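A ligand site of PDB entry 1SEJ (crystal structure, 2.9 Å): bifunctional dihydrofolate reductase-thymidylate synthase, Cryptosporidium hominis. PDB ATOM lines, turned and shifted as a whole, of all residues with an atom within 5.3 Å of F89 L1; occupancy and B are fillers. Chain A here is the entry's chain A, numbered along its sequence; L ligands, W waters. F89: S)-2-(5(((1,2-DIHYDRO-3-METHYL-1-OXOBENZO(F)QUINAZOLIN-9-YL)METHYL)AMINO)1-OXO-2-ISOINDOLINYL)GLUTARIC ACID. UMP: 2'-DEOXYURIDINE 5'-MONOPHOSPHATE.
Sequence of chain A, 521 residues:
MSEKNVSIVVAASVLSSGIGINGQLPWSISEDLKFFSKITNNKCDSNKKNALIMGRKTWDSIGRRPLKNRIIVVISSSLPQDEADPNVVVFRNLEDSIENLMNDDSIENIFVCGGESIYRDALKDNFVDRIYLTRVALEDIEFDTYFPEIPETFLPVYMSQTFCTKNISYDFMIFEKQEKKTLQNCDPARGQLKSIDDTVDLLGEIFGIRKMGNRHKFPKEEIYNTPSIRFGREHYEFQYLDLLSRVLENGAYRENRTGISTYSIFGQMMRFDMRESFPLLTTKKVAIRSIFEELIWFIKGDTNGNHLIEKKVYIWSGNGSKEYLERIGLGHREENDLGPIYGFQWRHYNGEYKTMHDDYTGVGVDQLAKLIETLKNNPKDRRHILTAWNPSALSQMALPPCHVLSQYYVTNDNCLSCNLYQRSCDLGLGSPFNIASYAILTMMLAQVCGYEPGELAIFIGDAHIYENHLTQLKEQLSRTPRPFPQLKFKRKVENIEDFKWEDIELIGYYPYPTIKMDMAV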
ATOM      1  N   ARG A 257     -15.087  29.141  26.417  1.00  0.00           N
ATOM      2  CA  ARG A 257     -16.184  29.013  25.454  1.00  0.00           C
ATOM      3  C   ARG A 257     -16.965  27.693  25.543  1.00  0.00           C
ATOM      4  O   ARG A 257     -18.177  27.671  25.337  1.00  0.00           O
ATOM      5  CB  ARG A 257     -15.655  29.230  24.028  1.00  0.00           C
ATOM      6  CG  ARG A 257     -14.588  28.287  23.600  1.00  0.00           C
ATOM      7  CD  ARG A 257     -14.655  28.108  22.104  1.00  0.00           C
ATOM      8  NE  ARG A 257     -14.036  26.848  21.787  1.00  0.00           N
ATOM      9  CZ  ARG A 257     -14.574  25.736  21.311  1.00  0.00           C
ATOM     10  NH1 ARG A 257     -13.742  24.725  21.149  1.00  0.00           N
ATOM     11  NH2 ARG A 257     -15.846  25.604  20.969  1.00  0.00           N
ATOM     12  N   THR A 258     -16.269  26.593  25.834  1.00  0.00           N
ATOM     13  CA  THR A 258     -16.961  25.307  25.964  1.00  0.00           C
ATOM     14  C   THR A 258     -17.589  25.297  27.345  1.00  0.00           C
ATOM     15  O   THR A 258     -17.262  26.127  28.191  1.00  0.00           O
ATOM     16  CB  THR A 258     -15.987  24.094  25.843  1.00  0.00           C
ATOM     17  OG1 THR A 258     -15.464  23.760  27.135  1.00  0.00           O
ATOM     18  CG2 THR A 258     -14.837  24.428  24.893  1.00  0.00           C
ATOM     19  N   ALA A 287      -3.836   6.902  18.829  1.00  0.00           N
ATOM     20  CA  ALA A 287      -4.265   6.545  17.478  1.00  0.00           C
ATOM     21  C   ALA A 287      -3.445   7.245  16.400  1.00  0.00           C
ATOM     22  O   ALA A 287      -3.812   8.337  15.941  1.00  0.00           O
ATOM     23  CB  ALA A 287      -5.749   6.847  17.291  1.00  0.00           C
ATOM     24  N   SER A 290      -5.355   8.035  12.828  1.00  0.00           N
ATOM     25  CA  SER A 290      -6.185   9.230  12.845  1.00  0.00           C
ATOM     26  C   SER A 290      -5.309  10.483  12.662  1.00  0.00           C
ATOM     27  O   SER A 290      -5.630  11.372  11.869  1.00  0.00           O
ATOM     28  CB  SER A 290      -6.958   9.307  14.171  1.00  0.00           C
ATOM     29  OG  SER A 290      -7.718   8.128  14.388  1.00  0.00           O
ATOM     30  N   ILE A 291      -4.204  10.542  13.412  1.00  0.00           N
ATOM     31  CA  ILE A 291      -3.260  11.657  13.340  1.00  0.00           C
ATOM     32  C   ILE A 291      -2.849  11.862  11.884  1.00  0.00           C
ATOM     33  O   ILE A 291      -3.042  12.934  11.317  1.00  0.00           O
ATOM     34  CB  ILE A 291      -1.986  11.371  14.167  1.00  0.00           C
ATOM     35  CG1 ILE A 291      -2.341  11.254  15.643  1.00  0.00           C
ATOM     36  CG2 ILE A 291      -0.950  12.463  13.975  1.00  0.00           C
ATOM     37  CD1 ILE A 291      -1.162  10.852  16.502  1.00  0.00           C
ATOM     38  N   GLU A 294      -5.415  13.203   9.470  1.00  0.00           N
ATOM     39  CA  GLU A 294      -5.730  14.625   9.620  1.00  0.00           C
ATOM     40  C   GLU A 294      -4.607  15.453   9.000  1.00  0.00           C
ATOM     41  O   GLU A 294      -4.846  16.510   8.444  1.00  0.00           O
ATOM     42  CB  GLU A 294      -5.889  15.021  11.094  1.00  0.00           C
ATOM     43  CG  GLU A 294      -6.050  16.538  11.288  1.00  0.00           C
ATOM     44  CD  GLU A 294      -5.962  16.969  12.742  1.00  0.00           C
ATOM     45  OE1 GLU A 294      -4.952  16.619  13.411  1.00  0.00           O
ATOM     46  OE2 GLU A 294      -6.878  17.659  13.213  1.00  0.00           O
ATOM     47  N   VAL A 313     -12.336   9.314  10.989  1.00  0.00           N
ATOM     48  CA  VAL A 313     -11.659  10.221  11.919  1.00  0.00           C
ATOM     49  C   VAL A 313     -12.761  11.204  12.269  1.00  0.00           C
ATOM     50  O   VAL A 313     -13.285  11.882  11.393  1.00  0.00           O
ATOM     51  CB  VAL A 313     -10.497  10.982  11.254  1.00  0.00           C
ATOM     52  CG1 VAL A 313      -9.864  11.931  12.257  1.00  0.00           C
ATOM     53  CG2 VAL A 313      -9.448  10.000  10.747  1.00  0.00           C
ATOM     54  N   TYR A 314     -13.095  11.292  13.557  1.00  0.00           N
ATOM     55  CA  TYR A 314     -14.202  12.142  13.961  1.00  0.00           C
ATOM     56  C   TYR A 314     -13.949  13.379  14.822  1.00  0.00           C
ATOM     57  O   TYR A 314     -14.904  13.969  15.334  1.00  0.00           O
ATOM     58  CB  TYR A 314     -15.242  11.267  14.668  1.00  0.00           C
ATOM     59  CG  TYR A 314     -15.542   9.968  13.959  1.00  0.00           C
ATOM     60  CD1 TYR A 314     -16.256   9.949  12.765  1.00  0.00           C
ATOM     61  CD2 TYR A 314     -15.091   8.748  14.478  1.00  0.00           C
ATOM     62  CE1 TYR A 314     -16.521   8.762  12.094  1.00  0.00           C
ATOM     63  CE2 TYR A 314     -15.346   7.553  13.813  1.00  0.00           C
ATOM     64  CZ  TYR A 314     -16.069   7.562  12.622  1.00  0.00           C
ATOM     65  OH  TYR A 314     -16.315   6.390  11.957  1.00  0.00           O
ATOM     66  N   ILE A 315     -12.708  13.793  14.988  1.00  0.00           N
ATOM     67  CA  ILE A 315     -12.459  14.945  15.843  1.00  0.00           C
ATOM     68  C   ILE A 315     -13.091  16.240  15.380  1.00  0.00           C
ATOM     69  O   ILE A 315     -13.492  17.061  16.212  1.00  0.00           O
ATOM     70  CB  ILE A 315     -10.977  15.211  16.013  1.00  0.00           C
ATOM     71  CG1 ILE A 315     -10.307  15.234  14.642  1.00  0.00           C
ATOM     72  CG2 ILE A 315     -10.399  14.157  16.921  1.00  0.00           C
ATOM     73  CD1 ILE A 315      -8.859  15.661  14.683  1.00  0.00           C
ATOM     74  N   TRP A 316     -13.174  16.447  14.069  1.00  0.00           N
ATOM     75  CA  TRP A 316     -13.745  17.673  13.550  1.00  0.00           C
ATOM     76  C   TRP A 316     -15.264  17.638  13.366  1.00  0.00           C
ATOM     77  O   TRP A 316     -15.851  18.577  12.829  1.00  0.00           O
ATOM     78  CB  TRP A 316     -13.077  18.077  12.242  1.00  0.00           C
ATOM     79  CG  TRP A 316     -11.672  18.561  12.413  1.00  0.00           C
ATOM     80  CD1 TRP A 316     -10.524  17.826  12.340  1.00  0.00           C
ATOM     81  CD2 TRP A 316     -11.268  19.902  12.721  1.00  0.00           C
ATOM     82  NE1 TRP A 316      -9.428  18.629  12.578  1.00  0.00           N
ATOM     83  CE2 TRP A 316      -9.865  19.900  12.817  1.00  0.00           C
ATOM     84  CE3 TRP A 316     -11.959  21.098  12.936  1.00  0.00           C
ATOM     85  CZ2 TRP A 316      -9.138  21.059  13.102  1.00  0.00           C
ATOM     86  CZ3 TRP A 316     -11.235  22.245  13.227  1.00  0.00           C
ATOM     87  CH2 TRP A 316      -9.841  22.220  13.309  1.00  0.00           C
ATOM     88  N   ASN A 319     -17.049  20.372  15.872  1.00  0.00           N
ATOM     89  CA  ASN A 319     -16.986  21.729  15.336  1.00  0.00           C
ATOM     90  C   ASN A 319     -17.437  21.807  13.882  1.00  0.00           C
ATOM     91  O   ASN A 319     -17.329  22.852  13.249  1.00  0.00           O
ATOM     92  CB  ASN A 319     -15.552  22.278  15.474  1.00  0.00           C
ATOM     93  CG  ASN A 319     -15.104  22.347  16.924  1.00  0.00           C
ATOM     94  OD1 ASN A 319     -14.892  21.312  17.584  1.00  0.00           O
ATOM     95  ND2 ASN A 319     -14.960  23.565  17.447  1.00  0.00           N
ATOM     96  N   LEU A 399     -13.265  27.017  13.718  1.00  0.00           N
ATOM     97  CA  LEU A 399     -12.450  27.097  14.918  1.00  0.00           C
ATOM     98  C   LEU A 399     -11.135  27.777  14.565  1.00  0.00           C
ATOM     99  O   LEU A 399     -10.482  27.407  13.583  1.00  0.00           O
ATOM    100  CB  LEU A 399     -12.185  25.693  15.454  1.00  0.00           C
ATOM    101  CG  LEU A 399     -11.660  25.556  16.881  1.00  0.00           C
ATOM    102  CD1 LEU A 399     -12.656  26.181  17.843  1.00  0.00           C
ATOM    103  CD2 LEU A 399     -11.467  24.078  17.207  1.00  0.00           C
ATOM    104  N   ASP A 426      -5.164  21.520  24.657  1.00  0.00           N
ATOM    105  CA  ASP A 426      -5.901  20.606  25.518  1.00  0.00           C
ATOM    106  C   ASP A 426      -4.936  19.468  25.846  1.00  0.00           C
ATOM    107  O   ASP A 426      -4.832  18.485  25.109  1.00  0.00           O
ATOM    108  CB  ASP A 426      -7.131  20.076  24.786  1.00  0.00           C
ATOM    109  CG  ASP A 426      -7.873  19.012  25.566  1.00  0.00           C
ATOM    110  OD1 ASP A 426      -9.009  18.665  25.164  1.00  0.00           O
ATOM    111  OD2 ASP A 426      -7.330  18.503  26.580  1.00  0.00           O
ATOM    112  N   LEU A 429      -6.575  15.734  25.829  1.00  0.00           N
ATOM    113  CA  LEU A 429      -7.074  15.164  24.600  1.00  0.00           C
ATOM    114  C   LEU A 429      -6.235  15.446  23.356  1.00  0.00           C
ATOM    115  O   LEU A 429      -5.812  14.510  22.684  1.00  0.00           O
ATOM    116  CB  LEU A 429      -8.504  15.635  24.368  1.00  0.00           C
ATOM    117  CG  LEU A 429      -9.267  14.942  23.249  1.00  0.00           C
ATOM    118  CD1 LEU A 429      -9.322  13.435  23.530  1.00  0.00           C
ATOM    119  CD2 LEU A 429     -10.674  15.530  23.165  1.00  0.00           C
ATOM    120  N   GLY A 430      -6.011  16.722  23.059  1.00  0.00           N
ATOM    121  CA  GLY A 430      -5.268  17.085  21.860  1.00  0.00           C
ATOM    122  C   GLY A 430      -3.755  17.011  21.860  1.00  0.00           C
ATOM    123  O   GLY A 430      -3.153  16.427  20.963  1.00  0.00           O
ATOM    124  N   PHE A 433      -1.765  14.240  20.411  1.00  0.00           N
ATOM    125  CA  PHE A 433      -1.895  14.183  18.974  1.00  0.00           C
ATOM    126  C   PHE A 433      -1.101  15.275  18.283  1.00  0.00           C
ATOM    127  O   PHE A 433      -0.522  15.047  17.227  1.00  0.00           O
ATOM    128  CB  PHE A 433      -3.354  14.243  18.567  1.00  0.00           C
ATOM    129  CG  PHE A 433      -4.149  13.058  19.031  1.00  0.00           C
ATOM    130  CD1 PHE A 433      -4.515  12.933  20.365  1.00  0.00           C
ATOM    131  CD2 PHE A 433      -4.469  12.032  18.164  1.00  0.00           C
ATOM    132  CE1 PHE A 433      -5.187  11.785  20.831  1.00  0.00           C
ATOM    133  CE2 PHE A 433      -5.137  10.889  18.608  1.00  0.00           C
ATOM    134  CZ  PHE A 433      -5.495  10.765  19.949  1.00  0.00           C
ATOM    135  N   ASN A 434      -1.045  16.460  18.871  1.00  0.00           N
ATOM    136  CA  ASN A 434      -0.268  17.530  18.237  1.00  0.00           C
ATOM    137  C   ASN A 434       1.201  17.167  18.158  1.00  0.00           C
ATOM    138  O   ASN A 434       1.846  17.377  17.132  1.00  0.00           O
ATOM    139  CB  ASN A 434      -0.411  18.836  19.001  1.00  0.00           C
ATOM    140  CG  ASN A 434      -1.754  19.452  18.832  1.00  0.00           C
ATOM    141  OD1 ASN A 434      -2.680  19.183  19.610  1.00  0.00           O
ATOM    142  ND2 ASN A 434      -1.901  20.283  17.801  1.00  0.00           N
ATOM    143  N   TYR A 466      -8.962  19.971  30.980  1.00  0.00           N
ATOM    144  CA  TYR A 466     -10.400  20.087  31.196  1.00  0.00           C
ATOM    145  C   TYR A 466     -10.707  19.283  32.462  1.00  0.00           C
ATOM    146  O   TYR A 466     -10.199  18.178  32.647  1.00  0.00           O
ATOM    147  CB  TYR A 466     -11.161  19.551  29.987  1.00  0.00           C
ATOM    148  CG  TYR A 466     -11.196  20.533  28.845  1.00  0.00           C
ATOM    149  CD1 TYR A 466     -12.140  21.560  28.821  1.00  0.00           C
ATOM    150  CD2 TYR A 466     -10.224  20.493  27.841  1.00  0.00           C
ATOM    151  CE1 TYR A 466     -12.112  22.548  27.807  1.00  0.00           C
ATOM    152  CE2 TYR A 466     -10.193  21.471  26.826  1.00  0.00           C
ATOM    153  CZ  TYR A 466     -11.134  22.497  26.830  1.00  0.00           C
ATOM    154  OH  TYR A 466     -11.066  23.470  25.868  1.00  0.00           O
ATOM    155  N   MET A 517     -11.127   9.768  26.893  1.00  0.00           N
ATOM    156  CA  MET A 517     -11.271  11.146  27.354  1.00  0.00           C
ATOM    157  C   MET A 517     -12.152  11.923  26.407  1.00  0.00           C
ATOM    158  O   MET A 517     -11.805  12.110  25.236  1.00  0.00           O
ATOM    159  CB  MET A 517      -9.914  11.812  27.459  1.00  0.00           C
ATOM    160  CG  MET A 517      -9.050  11.197  28.527  1.00  0.00           C
ATOM    161  SD  MET A 517      -7.457  11.950  28.580  1.00  0.00           S
ATOM    162  CE  MET A 517      -6.690  11.104  27.160  1.00  0.00           C
ATOM    163  N   MET A 519     -14.182  15.056  24.594  1.00  0.00           N
ATOM    164  CA  MET A 519     -13.992  16.442  24.152  1.00  0.00           C
ATOM    165  C   MET A 519     -15.183  17.354  24.514  1.00  0.00           C
ATOM    166  O   MET A 519     -16.320  16.897  24.662  1.00  0.00           O
ATOM    167  CB  MET A 519     -13.810  16.478  22.634  1.00  0.00           C
ATOM    168  CG  MET A 519     -13.737  17.885  22.058  1.00  0.00           C
ATOM    169  SD  MET A 519     -13.949  17.977  20.269  1.00  0.00           S
ATOM    170  CE  MET A 519     -15.621  18.752  20.137  1.00  0.00           C
ATOM    171  N   ALA A 520     -14.907  18.652  24.670  1.00  0.00           N
ATOM    172  CA  ALA A 520     -15.941  19.639  24.969  1.00  0.00           C
ATOM    173  C   ALA A 520     -16.196  20.363  23.635  1.00  0.00           C
ATOM    174  O   ALA A 520     -15.273  20.938  23.050  1.00  0.00           O
ATOM    175  CB  ALA A 520     -15.444  20.614  26.032  1.00  0.00           C
HETATM  176  C1  F89 L   1      -9.301  19.221  21.319  1.00  0.00           C
HETATM  177  O1A F89 L   1      -8.256  18.591  21.450  1.00  0.00           O
HETATM  178  N2  F89 L   1      -9.964  19.654  22.484  1.00  0.00           N
HETATM  179  C3  F89 L   1     -11.165  20.360  22.376  1.00  0.00           C
HETATM  180  C3M F89 L   1     -11.906  20.832  23.625  1.00  0.00           C
HETATM  181  N4  F89 L   1     -11.665  20.619  21.155  1.00  0.00           N
HETATM  182  C4A F89 L   1     -11.046  20.222  20.033  1.00  0.00           C
HETATM  183  C5  F89 L   1     -11.639  20.546  18.827  1.00  0.00           C
HETATM  184  C6  F89 L   1     -10.951  20.113  17.537  1.00  0.00           C
HETATM  185  C6A F89 L   1      -9.758  19.406  17.639  1.00  0.00           C
HETATM  186  C7  F89 L   1      -9.111  19.022  16.464  1.00  0.00           C
HETATM  187  C8  F89 L   1      -7.909  18.321  16.522  1.00  0.00           C
HETATM  188  C9  F89 L   1      -7.356  18.014  17.755  1.00  0.00           C
HETATM  189  C10 F89 L   1      -7.999  18.410  18.923  1.00  0.00           C
HETATM  190  C1B F89 L   1      -9.206  19.107  18.887  1.00  0.00           C
HETATM  191  C1A F89 L   1      -9.837  19.515  20.068  1.00  0.00           C
HETATM  192  C11 F89 L   1      -6.043  17.221  17.815  1.00  0.00           C
HETATM  193  N12 F89 L   1      -6.071  16.129  16.823  1.00  0.00           N
HETATM  194  C13 F89 L   1      -6.611  14.941  17.063  1.00  0.00           C
HETATM  195  C14 F89 L   1      -7.245  14.661  18.284  1.00  0.00           C
HETATM  196  C15 F89 L   1      -7.883  13.438  18.476  1.00  0.00           C
HETATM  197  C16 F89 L   1      -7.882  12.483  17.461  1.00  0.00           C
HETATM  198  C17 F89 L   1      -7.244  12.752  16.254  1.00  0.00           C
HETATM  199  C18 F89 L   1      -6.606  13.976  16.062  1.00  0.00           C
HETATM  200  C19 F89 L   1      -8.571  12.941  19.502  1.00  0.00           C
HETATM  201  C   F89 L   1      -8.630  11.416  17.949  1.00  0.00           C
HETATM  202  O   F89 L   1      -8.885  10.383  17.337  1.00  0.00           O
HETATM  203  N   F89 L   1      -9.033  11.731  19.182  1.00  0.00           N
HETATM  204  CA  F89 L   1      -9.919  10.939  20.048  1.00  0.00           C
HETATM  205  CT  F89 L   1      -9.150   9.919  20.892  1.00  0.00           C
HETATM  206  O1  F89 L   1      -8.688   8.906  20.368  1.00  0.00           O
HETATM  207  O2  F89 L   1      -9.010  10.087  22.100  1.00  0.00           O
HETATM  208  CB  F89 L   1     -11.010  10.228  19.244  1.00  0.00           C
HETATM  209  CG  F89 L   1     -11.959  11.237  18.585  1.00  0.00           C
HETATM  210  CD  F89 L   1     -12.779  12.012  19.628  1.00  0.00           C
HETATM  211  OE1 F89 L   1     -12.325  12.200  20.757  1.00  0.00           O
HETATM  212  OE2 F89 L   1     -13.890  12.449  19.341  1.00  0.00           O
HETATM  213  N1  UMP L   2      -7.280  21.998  20.560  1.00  0.00           N
HETATM  214  C2  UMP L   2      -6.023  21.361  20.773  1.00  0.00           C
HETATM  215  N3  UMP L   2      -5.256  21.011  19.729  1.00  0.00           N
HETATM  216  C4  UMP L   2      -5.662  21.074  18.448  1.00  0.00           C
HETATM  217  C5  UMP L   2      -7.080  21.541  18.092  1.00  0.00           C
HETATM  218  C6  UMP L   2      -7.664  22.457  19.182  1.00  0.00           C
HETATM  219  O2  UMP L   2      -5.600  21.202  21.918  1.00  0.00           O
HETATM  220  O4  UMP L   2      -4.892  20.763  17.549  1.00  0.00           O
HETATM  221  C1' UMP L   2      -8.127  22.426  21.726  1.00  0.00           C
HETATM  222  C2' UMP L   2      -7.543  23.415  22.509  1.00  0.00           C
HETATM  223  C3' UMP L   2      -8.731  23.971  23.275  1.00  0.00           C
HETATM  224  C4' UMP L   2      -9.871  23.940  22.260  1.00  0.00           C
HETATM  225  O3' UMP L   2      -9.039  23.120  24.381  1.00  0.00           O
HETATM  226  O4' UMP L   2      -9.422  22.949  21.289  1.00  0.00           O
HETATM  227  C5' UMP L   2      -9.984  25.313  21.568  1.00  0.00           C
HETATM  228  O5' UMP L   2     -10.386  26.311  22.498  1.00  0.00           O
HETATM  229  P   UMP L   2     -10.407  27.851  22.078  1.00  0.00           P
HETATM  230  OP1 UMP L   2     -11.364  27.871  20.816  1.00  0.00           O
HETATM  231  OP2 UMP L   2     -11.034  28.640  23.156  1.00  0.00           O
HETATM  232  OP3 UMP L   2      -9.061  28.236  21.622  1.00  0.00           O
HETATM  233  O   HOH W   1      -7.001   9.628  24.098  1.00  0.00           O
HETATM  234  O   HOH W   2      -5.666  19.611  14.765  1.00  0.00           O
HETATM  235  O   HOH W   3     -14.302  22.261  20.576  1.00  0.00           O
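Water W2 bridges the side-chain carboxylate of Glu 294 (2.8 Å) and an oxygen (O4) of UMP L2 (3.1 Å). Water W3 lies within hydrogen-bond range of NH1 of Arg 257 (2.6 Å), O of Ala 520 (3.0 Å), N4 of F89 L1 (3.2 Å) and OD1 of Asn 319 (3.2 Å).
Ser 290 touches F89 L1. Glu 294 touches F89 L1 (OE2 to C8, 3.5 Å). CG2 of Ile 315 touches C15 of F89 L1 (3.0 Å). Trp 316 touches F89 L1 (CE2 to C7, 3.8 Å). Asn 319 touches F89 L1 (OD1 to C5, 3.6 Å). Leu 399 touches F89 L1 (CD2 to C5, 3.9 Å). Leu 429 touches F89 L1. Phe 433 touches F89 L1. OH of Tyr 466 touches C3M of F89 L1 (3.6 Å). Ala 520 touches F89 L1. Hydrophobic or aromatic side chains within 4 Å of F89 L1: Ile 315, Trp 316, Leu 399, Leu 429, Phe 433, Tyr 466 and Met 519. 13 residues have an atom within 4 Å of F89 L1: Ser 290, Glu 294, Ile 315, Trp 316, Asn 319, Leu 399, Asp 426, Leu 429, Gly 430, Phe 433, Tyr 466, Met 519 and Ala 520. The nearest printed residue that does not touch F89 L1 is Asn 434 (4.3 Å).
OD2 of Asp 426 lies within hydrogen-bond range of N of Leu 429 (3.0 Å). O of Gly 430 sits close to OD1 of Asn 434 (3.1 Å). NE1 of Trp 316 lies within hydrogen-bond range of OE2 of Glu 294 (2.8 Å).
A nitrogen (N2) of F89 L1 is in hydrogen-bond range of the side-chain carboxylate of Asp 426 (3.0 Å). N of Gly 430 sits at hydrogen-bond distance from O1A of F89 L1 (3.3 Å). SD of Met 519 lies close to N4 of F89 L1 (3.6 Å). An oxygen (O2) of UMP L2 is in hydrogen-bond range of the backbone NH (N) of Asp 426, at 2.8 Å. The side-chain hydroxyl (OH) of Tyr 466 is in hydrogen-bond range of an oxygen (O3') of UMP L2, 2.5 Å away. O4 of UMP L2 is in hydrogen-bond range of ND2 of Asn 434 (3.0 Å). An oxygen (OP1) of UMP L2 lies within salt-bridge range of the guanidinium group (NE) of Arg 257 (3.0 Å).
A nitrogen (N4) of F89 L1 lies close to an oxygen (O4') of UMP L2, 3.2 Å away.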
